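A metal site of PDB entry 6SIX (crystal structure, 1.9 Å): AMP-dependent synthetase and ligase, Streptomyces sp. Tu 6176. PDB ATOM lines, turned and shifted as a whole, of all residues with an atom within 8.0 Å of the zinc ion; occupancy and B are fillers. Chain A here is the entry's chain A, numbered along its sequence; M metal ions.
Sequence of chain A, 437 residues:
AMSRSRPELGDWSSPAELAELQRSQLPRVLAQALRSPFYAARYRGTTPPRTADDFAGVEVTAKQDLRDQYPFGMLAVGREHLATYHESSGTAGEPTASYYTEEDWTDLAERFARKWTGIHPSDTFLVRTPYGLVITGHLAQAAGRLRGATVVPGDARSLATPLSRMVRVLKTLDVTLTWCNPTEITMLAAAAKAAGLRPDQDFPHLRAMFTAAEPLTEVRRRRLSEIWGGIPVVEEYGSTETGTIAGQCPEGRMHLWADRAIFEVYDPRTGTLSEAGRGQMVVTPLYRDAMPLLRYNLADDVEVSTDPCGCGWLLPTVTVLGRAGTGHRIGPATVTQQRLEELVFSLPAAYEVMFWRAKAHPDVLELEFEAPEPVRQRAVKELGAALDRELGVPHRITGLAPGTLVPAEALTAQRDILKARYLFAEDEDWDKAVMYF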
ATOM      1  N   GLY A 247     -14.279  15.503  -6.635  1.00  0.00           N
ATOM      2  CA  GLY A 247     -13.407  15.567  -7.821  1.00  0.00           C
ATOM      3  C   GLY A 247     -13.734  14.457  -8.810  1.00  0.00           C
ATOM      4  O   GLY A 247     -14.157  13.376  -8.378  1.00  0.00           O
ATOM      5  N   GLN A 248     -13.500  14.716 -10.087  1.00  0.00           N
ATOM      6  CA  GLN A 248     -13.742  13.788 -11.219  1.00  0.00           C
ATOM      7  C   GLN A 248     -12.839  12.563 -11.087  1.00  0.00           C
ATOM      8  O   GLN A 248     -11.685  12.710 -10.666  1.00  0.00           O
ATOM      9  CB  GLN A 248     -13.460  14.535 -12.517  1.00  0.00           C
ATOM     10  CG  GLN A 248     -14.047  13.881 -13.755  1.00  0.00           C
ATOM     11  CD  GLN A 248     -13.552  14.614 -14.973  1.00  0.00           C
ATOM     12  OE1 GLN A 248     -12.446  14.354 -15.482  1.00  0.00           O
ATOM     13  NE2 GLN A 248     -14.332  15.559 -15.437  1.00  0.00           N
ATOM     14  N   CYS A 249     -13.357  11.384 -11.407  1.00  0.00           N
ATOM     15  CA  CYS A 249     -12.566  10.141 -11.645  1.00  0.00           C
ATOM     16  C   CYS A 249     -12.318  10.010 -13.148  1.00  0.00           C
ATOM     17  O   CYS A 249     -12.896  10.752 -13.939  1.00  0.00           O
ATOM     18  CB  CYS A 249     -13.315   8.916 -11.126  1.00  0.00           C
ATOM     19  SG  CYS A 249     -14.711   8.477 -12.182  1.00  0.00           S
ATOM     20  N   PRO A 250     -11.472   9.061 -13.596  1.00  0.00           N
ATOM     21  CA  PRO A 250     -11.226   8.885 -15.024  1.00  0.00           C
ATOM     22  C   PRO A 250     -12.468   8.522 -15.853  1.00  0.00           C
ATOM     23  O   PRO A 250     -12.428   8.698 -17.043  1.00  0.00           O
ATOM     24  CB  PRO A 250     -10.193   7.731 -15.068  1.00  0.00           C
ATOM     25  CG  PRO A 250      -9.533   7.768 -13.704  1.00  0.00           C
ATOM     26  CD  PRO A 250     -10.642   8.166 -12.761  1.00  0.00           C
ATOM     27  N   GLU A 251     -13.547   8.061 -15.228  1.00  0.00           N
ATOM     28  CA  GLU A 251     -14.827   7.715 -15.915  1.00  0.00           C
ATOM     29  C   GLU A 251     -15.712   8.961 -16.067  1.00  0.00           C
ATOM     30  O   GLU A 251     -16.780   8.820 -16.665  1.00  0.00           O
ATOM     31  CB  GLU A 251     -15.602   6.645 -15.155  1.00  0.00           C
ATOM     32  CG  GLU A 251     -14.829   5.356 -14.920  1.00  0.00           C
ATOM     33  CD  GLU A 251     -14.193   4.755 -16.173  1.00  0.00           C
ATOM     34  OE1 GLU A 251     -13.022   4.368 -16.105  1.00  0.00           O
ATOM     35  OE2 GLU A 251     -14.877   4.685 -17.219  1.00  0.00           O
ATOM     36  N   GLY A 252     -15.333  10.120 -15.524  1.00  0.00           N
ATOM     37  CA  GLY A 252     -15.991  11.408 -15.775  1.00  0.00           C
ATOM     38  C   GLY A 252     -17.069  11.734 -14.751  1.00  0.00           C
ATOM     39  O   GLY A 252     -17.783  12.712 -14.977  1.00  0.00           O
ATOM     40  N   ARG A 253     -17.179  10.967 -13.676  1.00  0.00           N
ATOM     41  CA  ARG A 253     -18.090  11.269 -12.534  1.00  0.00           C
ATOM     42  C   ARG A 253     -17.311  11.963 -11.410  1.00  0.00           C
ATOM     43  O   ARG A 253     -16.120  11.608 -11.190  1.00  0.00           O
ATOM     44  CB  ARG A 253     -18.738   9.985 -12.033  1.00  0.00           C
ATOM     45  CG  ARG A 253     -19.588   9.262 -13.078  1.00  0.00           C
ATOM     46  CD  ARG A 253     -20.758   8.508 -12.475  1.00  0.00           C
ATOM     47  NE  ARG A 253     -21.337   7.538 -13.397  1.00  0.00           N
ATOM     48  CZ  ARG A 253     -20.815   6.342 -13.671  1.00  0.00           C
ATOM     49  NH1 ARG A 253     -19.688   5.947 -13.102  1.00  0.00           N
ATOM     50  NH2 ARG A 253     -21.420   5.529 -14.519  1.00  0.00           N
ATOM     51  N   MET A 254     -17.936  12.913 -10.718  1.00  0.00           N
ATOM     52  CA  MET A 254     -17.361  13.550  -9.520  1.00  0.00           C
ATOM     53  C   MET A 254     -17.656  12.668  -8.308  1.00  0.00           C
ATOM     54  O   MET A 254     -18.830  12.307  -8.125  1.00  0.00           O
ATOM     55  CB  MET A 254     -17.913  14.960  -9.286  1.00  0.00           C
ATOM     56  CG  MET A 254     -17.355  15.987 -10.272  1.00  0.00           C
ATOM     57  SD  MET A 254     -17.711  17.692  -9.758  1.00  0.00           S
ATOM     58  CE  MET A 254     -19.502  17.720  -9.904  1.00  0.00           C
ATOM     59  N   HIS A 255     -16.629  12.350  -7.523  1.00  0.00           N
ATOM     60  CA  HIS A 255     -16.763  11.554  -6.282  1.00  0.00           C
ATOM     61  C   HIS A 255     -16.584  12.489  -5.092  1.00  0.00           C
ATOM     62  O   HIS A 255     -15.653  13.288  -5.093  1.00  0.00           O
ATOM     63  CB  HIS A 255     -15.771  10.395  -6.281  1.00  0.00           C
ATOM     64  CG  HIS A 255     -16.090   9.307  -7.246  1.00  0.00           C
ATOM     65  ND1 HIS A 255     -16.659   8.102  -6.843  1.00  0.00           N
ATOM     66  CD2 HIS A 255     -15.904   9.195  -8.586  1.00  0.00           C
ATOM     67  CE1 HIS A 255     -16.801   7.319  -7.885  1.00  0.00           C
ATOM     68  NE2 HIS A 255     -16.356   7.950  -8.965  1.00  0.00           N
ATOM     69  N   ASP A 307     -23.967   4.080  -6.097  1.00  0.00           N
ATOM     70  CA  ASP A 307     -23.722   3.053  -7.135  1.00  0.00           C
ATOM     71  C   ASP A 307     -22.225   2.971  -7.429  1.00  0.00           C
ATOM     72  O   ASP A 307     -21.578   3.993  -7.620  1.00  0.00           O
ATOM     73  CB  ASP A 307     -24.457   3.366  -8.446  1.00  0.00           C
ATOM     74  CG  ASP A 307     -25.968   3.212  -8.368  1.00  0.00           C
ATOM     75  OD1 ASP A 307     -26.441   2.584  -7.412  1.00  0.00           O
ATOM     76  OD2 ASP A 307     -26.638   3.736  -9.276  1.00  0.00           O
ATOM     77  N   PRO A 308     -21.628   1.751  -7.474  1.00  0.00           N
ATOM     78  CA  PRO A 308     -20.189   1.649  -7.741  1.00  0.00           C
ATOM     79  C   PRO A 308     -19.853   2.219  -9.124  1.00  0.00           C
ATOM     80  O   PRO A 308     -20.712   2.212 -10.015  1.00  0.00           O
ATOM     81  CB  PRO A 308     -19.867   0.146  -7.648  1.00  0.00           C
ATOM     82  CG  PRO A 308     -21.221  -0.569  -7.673  1.00  0.00           C
ATOM     83  CD  PRO A 308     -22.266   0.451  -7.252  1.00  0.00           C
ATOM     84  N   CYS A 309     -18.630   2.742  -9.264  1.00  0.00           N
ATOM     85  CA  CYS A 309     -18.129   3.350 -10.513  1.00  0.00           C
ATOM     86  C   CYS A 309     -16.985   2.476 -11.062  1.00  0.00           C
ATOM     87  O   CYS A 309     -16.248   1.903 -10.245  1.00  0.00           O
ATOM     88  CB  CYS A 309     -17.651   4.780 -10.255  1.00  0.00           C
ATOM     89  SG  CYS A 309     -17.314   5.711 -11.767  1.00  0.00           S
ATOM     90  N   GLY A 310     -16.860   2.410 -12.396  1.00  0.00           N
ATOM     91  CA  GLY A 310     -15.771   1.731 -13.125  1.00  0.00           C
ATOM     92  C   GLY A 310     -14.378   2.148 -12.680  1.00  0.00           C
ATOM     93  O   GLY A 310     -13.441   1.369 -12.885  1.00  0.00           O
ATOM     94  N   CYS A 311     -14.228   3.332 -12.059  1.00  0.00           N
ATOM     95  CA  CYS A 311     -12.933   3.855 -11.556  1.00  0.00           C
ATOM     96  C   CYS A 311     -12.439   3.037 -10.348  1.00  0.00           C
ATOM     97  O   CYS A 311     -11.234   3.062 -10.089  1.00  0.00           O
ATOM     98  CB  CYS A 311     -13.030   5.326 -11.168  1.00  0.00           C
ATOM     99  SG  CYS A 311     -14.099   5.681  -9.745  1.00  0.00           S
ATOM    100  N   GLY A 312     -13.349   2.380  -9.625  1.00  0.00           N
ATOM    101  CA  GLY A 312     -13.006   1.539  -8.461  1.00  0.00           C
ATOM    102  C   GLY A 312     -12.728   2.355  -7.218  1.00  0.00           C
ATOM    103  O   GLY A 312     -12.338   1.765  -6.219  1.00  0.00           O
ATOM    104  N   TRP A 313     -12.915   3.684  -7.232  1.00  0.00           N
ATOM    105  CA  TRP A 313     -12.880   4.503  -5.979  1.00  0.00           C
ATOM    106  C   TRP A 313     -14.120   4.159  -5.161  1.00  0.00           C
ATOM    107  O   TRP A 313     -15.230   4.193  -5.717  1.00  0.00           O
ATOM    108  CB  TRP A 313     -12.862   6.004  -6.265  1.00  0.00           C
ATOM    109  CG  TRP A 313     -11.717   6.516  -7.082  1.00  0.00           C
ATOM    110  CD1 TRP A 313     -10.615   5.832  -7.521  1.00  0.00           C
ATOM    111  CD2 TRP A 313     -11.563   7.870  -7.512  1.00  0.00           C
ATOM    112  NE1 TRP A 313      -9.787   6.684  -8.213  1.00  0.00           N
ATOM    113  CE2 TRP A 313     -10.354   7.936  -8.226  1.00  0.00           C
ATOM    114  CE3 TRP A 313     -12.342   9.016  -7.369  1.00  0.00           C
ATOM    115  CZ2 TRP A 313      -9.908   9.119  -8.818  1.00  0.00           C
ATOM    116  CZ3 TRP A 313     -11.896  10.191  -7.937  1.00  0.00           C
ATOM    117  CH2 TRP A 313     -10.700  10.240  -8.639  1.00  0.00           C
ATOM    118  N   LEU A 314     -13.939   3.868  -3.876  1.00  0.00           N
ATOM    119  CA  LEU A 314     -15.056   3.451  -2.986  1.00  0.00           C
ATOM    120  C   LEU A 314     -15.671   4.709  -2.355  1.00  0.00           C
ATOM    121  O   LEU A 314     -15.564   4.915  -1.128  1.00  0.00           O
ATOM    122  CB  LEU A 314     -14.485   2.447  -1.978  1.00  0.00           C
ATOM    123  CG  LEU A 314     -13.999   1.139  -2.617  1.00  0.00           C
ATOM    124  CD1 LEU A 314     -13.495   0.175  -1.559  1.00  0.00           C
ATOM    125  CD2 LEU A 314     -15.094   0.479  -3.470  1.00  0.00           C
ATOM    126  N   LEU A 315     -16.279   5.542  -3.195  1.00  0.00           N
ATOM    127  CA  LEU A 315     -16.829   6.866  -2.804  1.00  0.00           C
ATOM    128  C   LEU A 315     -18.101   7.132  -3.597  1.00  0.00           C
ATOM    129  O   LEU A 315     -18.117   6.906  -4.799  1.00  0.00           O
ATOM    130  CB  LEU A 315     -15.775   7.934  -3.112  1.00  0.00           C
ATOM    131  CG  LEU A 315     -14.568   7.958  -2.173  1.00  0.00           C
ATOM    132  CD1 LEU A 315     -13.520   8.930  -2.691  1.00  0.00           C
ATOM    133  CD2 LEU A 315     -14.999   8.347  -0.775  1.00  0.00           C
ATOM    134  N   PRO A 316     -19.157   7.703  -2.975  1.00  0.00           N
ATOM    135  CA  PRO A 316     -20.354   8.090  -3.715  1.00  0.00           C
ATOM    136  C   PRO A 316     -20.042   9.163  -4.759  1.00  0.00           C
ATOM    137  O   PRO A 316     -19.089   9.927  -4.586  1.00  0.00           O
ATOM    138  CB  PRO A 316     -21.320   8.683  -2.687  1.00  0.00           C
ATOM    139  CG  PRO A 316     -20.741   8.263  -1.344  1.00  0.00           C
ATOM    140  CD  PRO A 316     -19.243   8.053  -1.559  1.00  0.00           C
ATOM    141  N   THR A 317     -20.832   9.174  -5.836  1.00  0.00           N
ATOM    142  CA  THR A 317     -20.733  10.174  -6.919  1.00  0.00           C
ATOM    143  C   THR A 317     -21.769  11.262  -6.664  1.00  0.00           C
ATOM    144  O   THR A 317     -22.756  11.009  -5.964  1.00  0.00           O
ATOM    145  CB  THR A 317     -20.869   9.529  -8.303  1.00  0.00           C
ATOM    146  OG1 THR A 317     -22.185   9.015  -8.409  1.00  0.00           O
ATOM    147  CG2 THR A 317     -19.881   8.401  -8.540  1.00  0.00           C
HETATM  148 ZN    ZN M   1     -15.657   7.045 -10.652  1.00  0.00          ZN
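ND1 of His 255 lies within hydrogen-bond range of O of Leu 315, 2.8 Å away.
The backbone carbonyl oxygen (O) of Gly 247 lies within hydrogen-bond range of the backbone NH (N) of His 255, at 2.8 Å.
The side-chain sulfur (SG) of Cys 311 sits close to the backbone NH (N) of Trp 313, 3.4 Å away.
SG of Cys 249 lies close to O of Arg 253 (3.6 Å).
The side-chain sulfur of Cys 249 lies close to the backbone NH of Glu 251, 3.3 Å away.
The side-chain sulfur (SG) of Cys 249 sits close to the backbone NH (N) of Gly 252 (3.8 Å).
SG of Cys 309 lies close to NH1 of Arg 253 (2.7 Å).
Four residues have an atom within 4 Å of the zinc ion: Cys 249, His 255, Cys 309 and Cys 311.
The nearest printed residue that does not touch the zinc ion is Arg 253 (4.5 Å).
The zinc ion is bound by NE2 of His 255 (2.0 Å), SG of Cys 311 (2.3 Å), SG of Cys 249 (2.3 Å) and SG of Cys 309 (2.4 Å).
The zinc ion has four donor atoms within binding distance.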
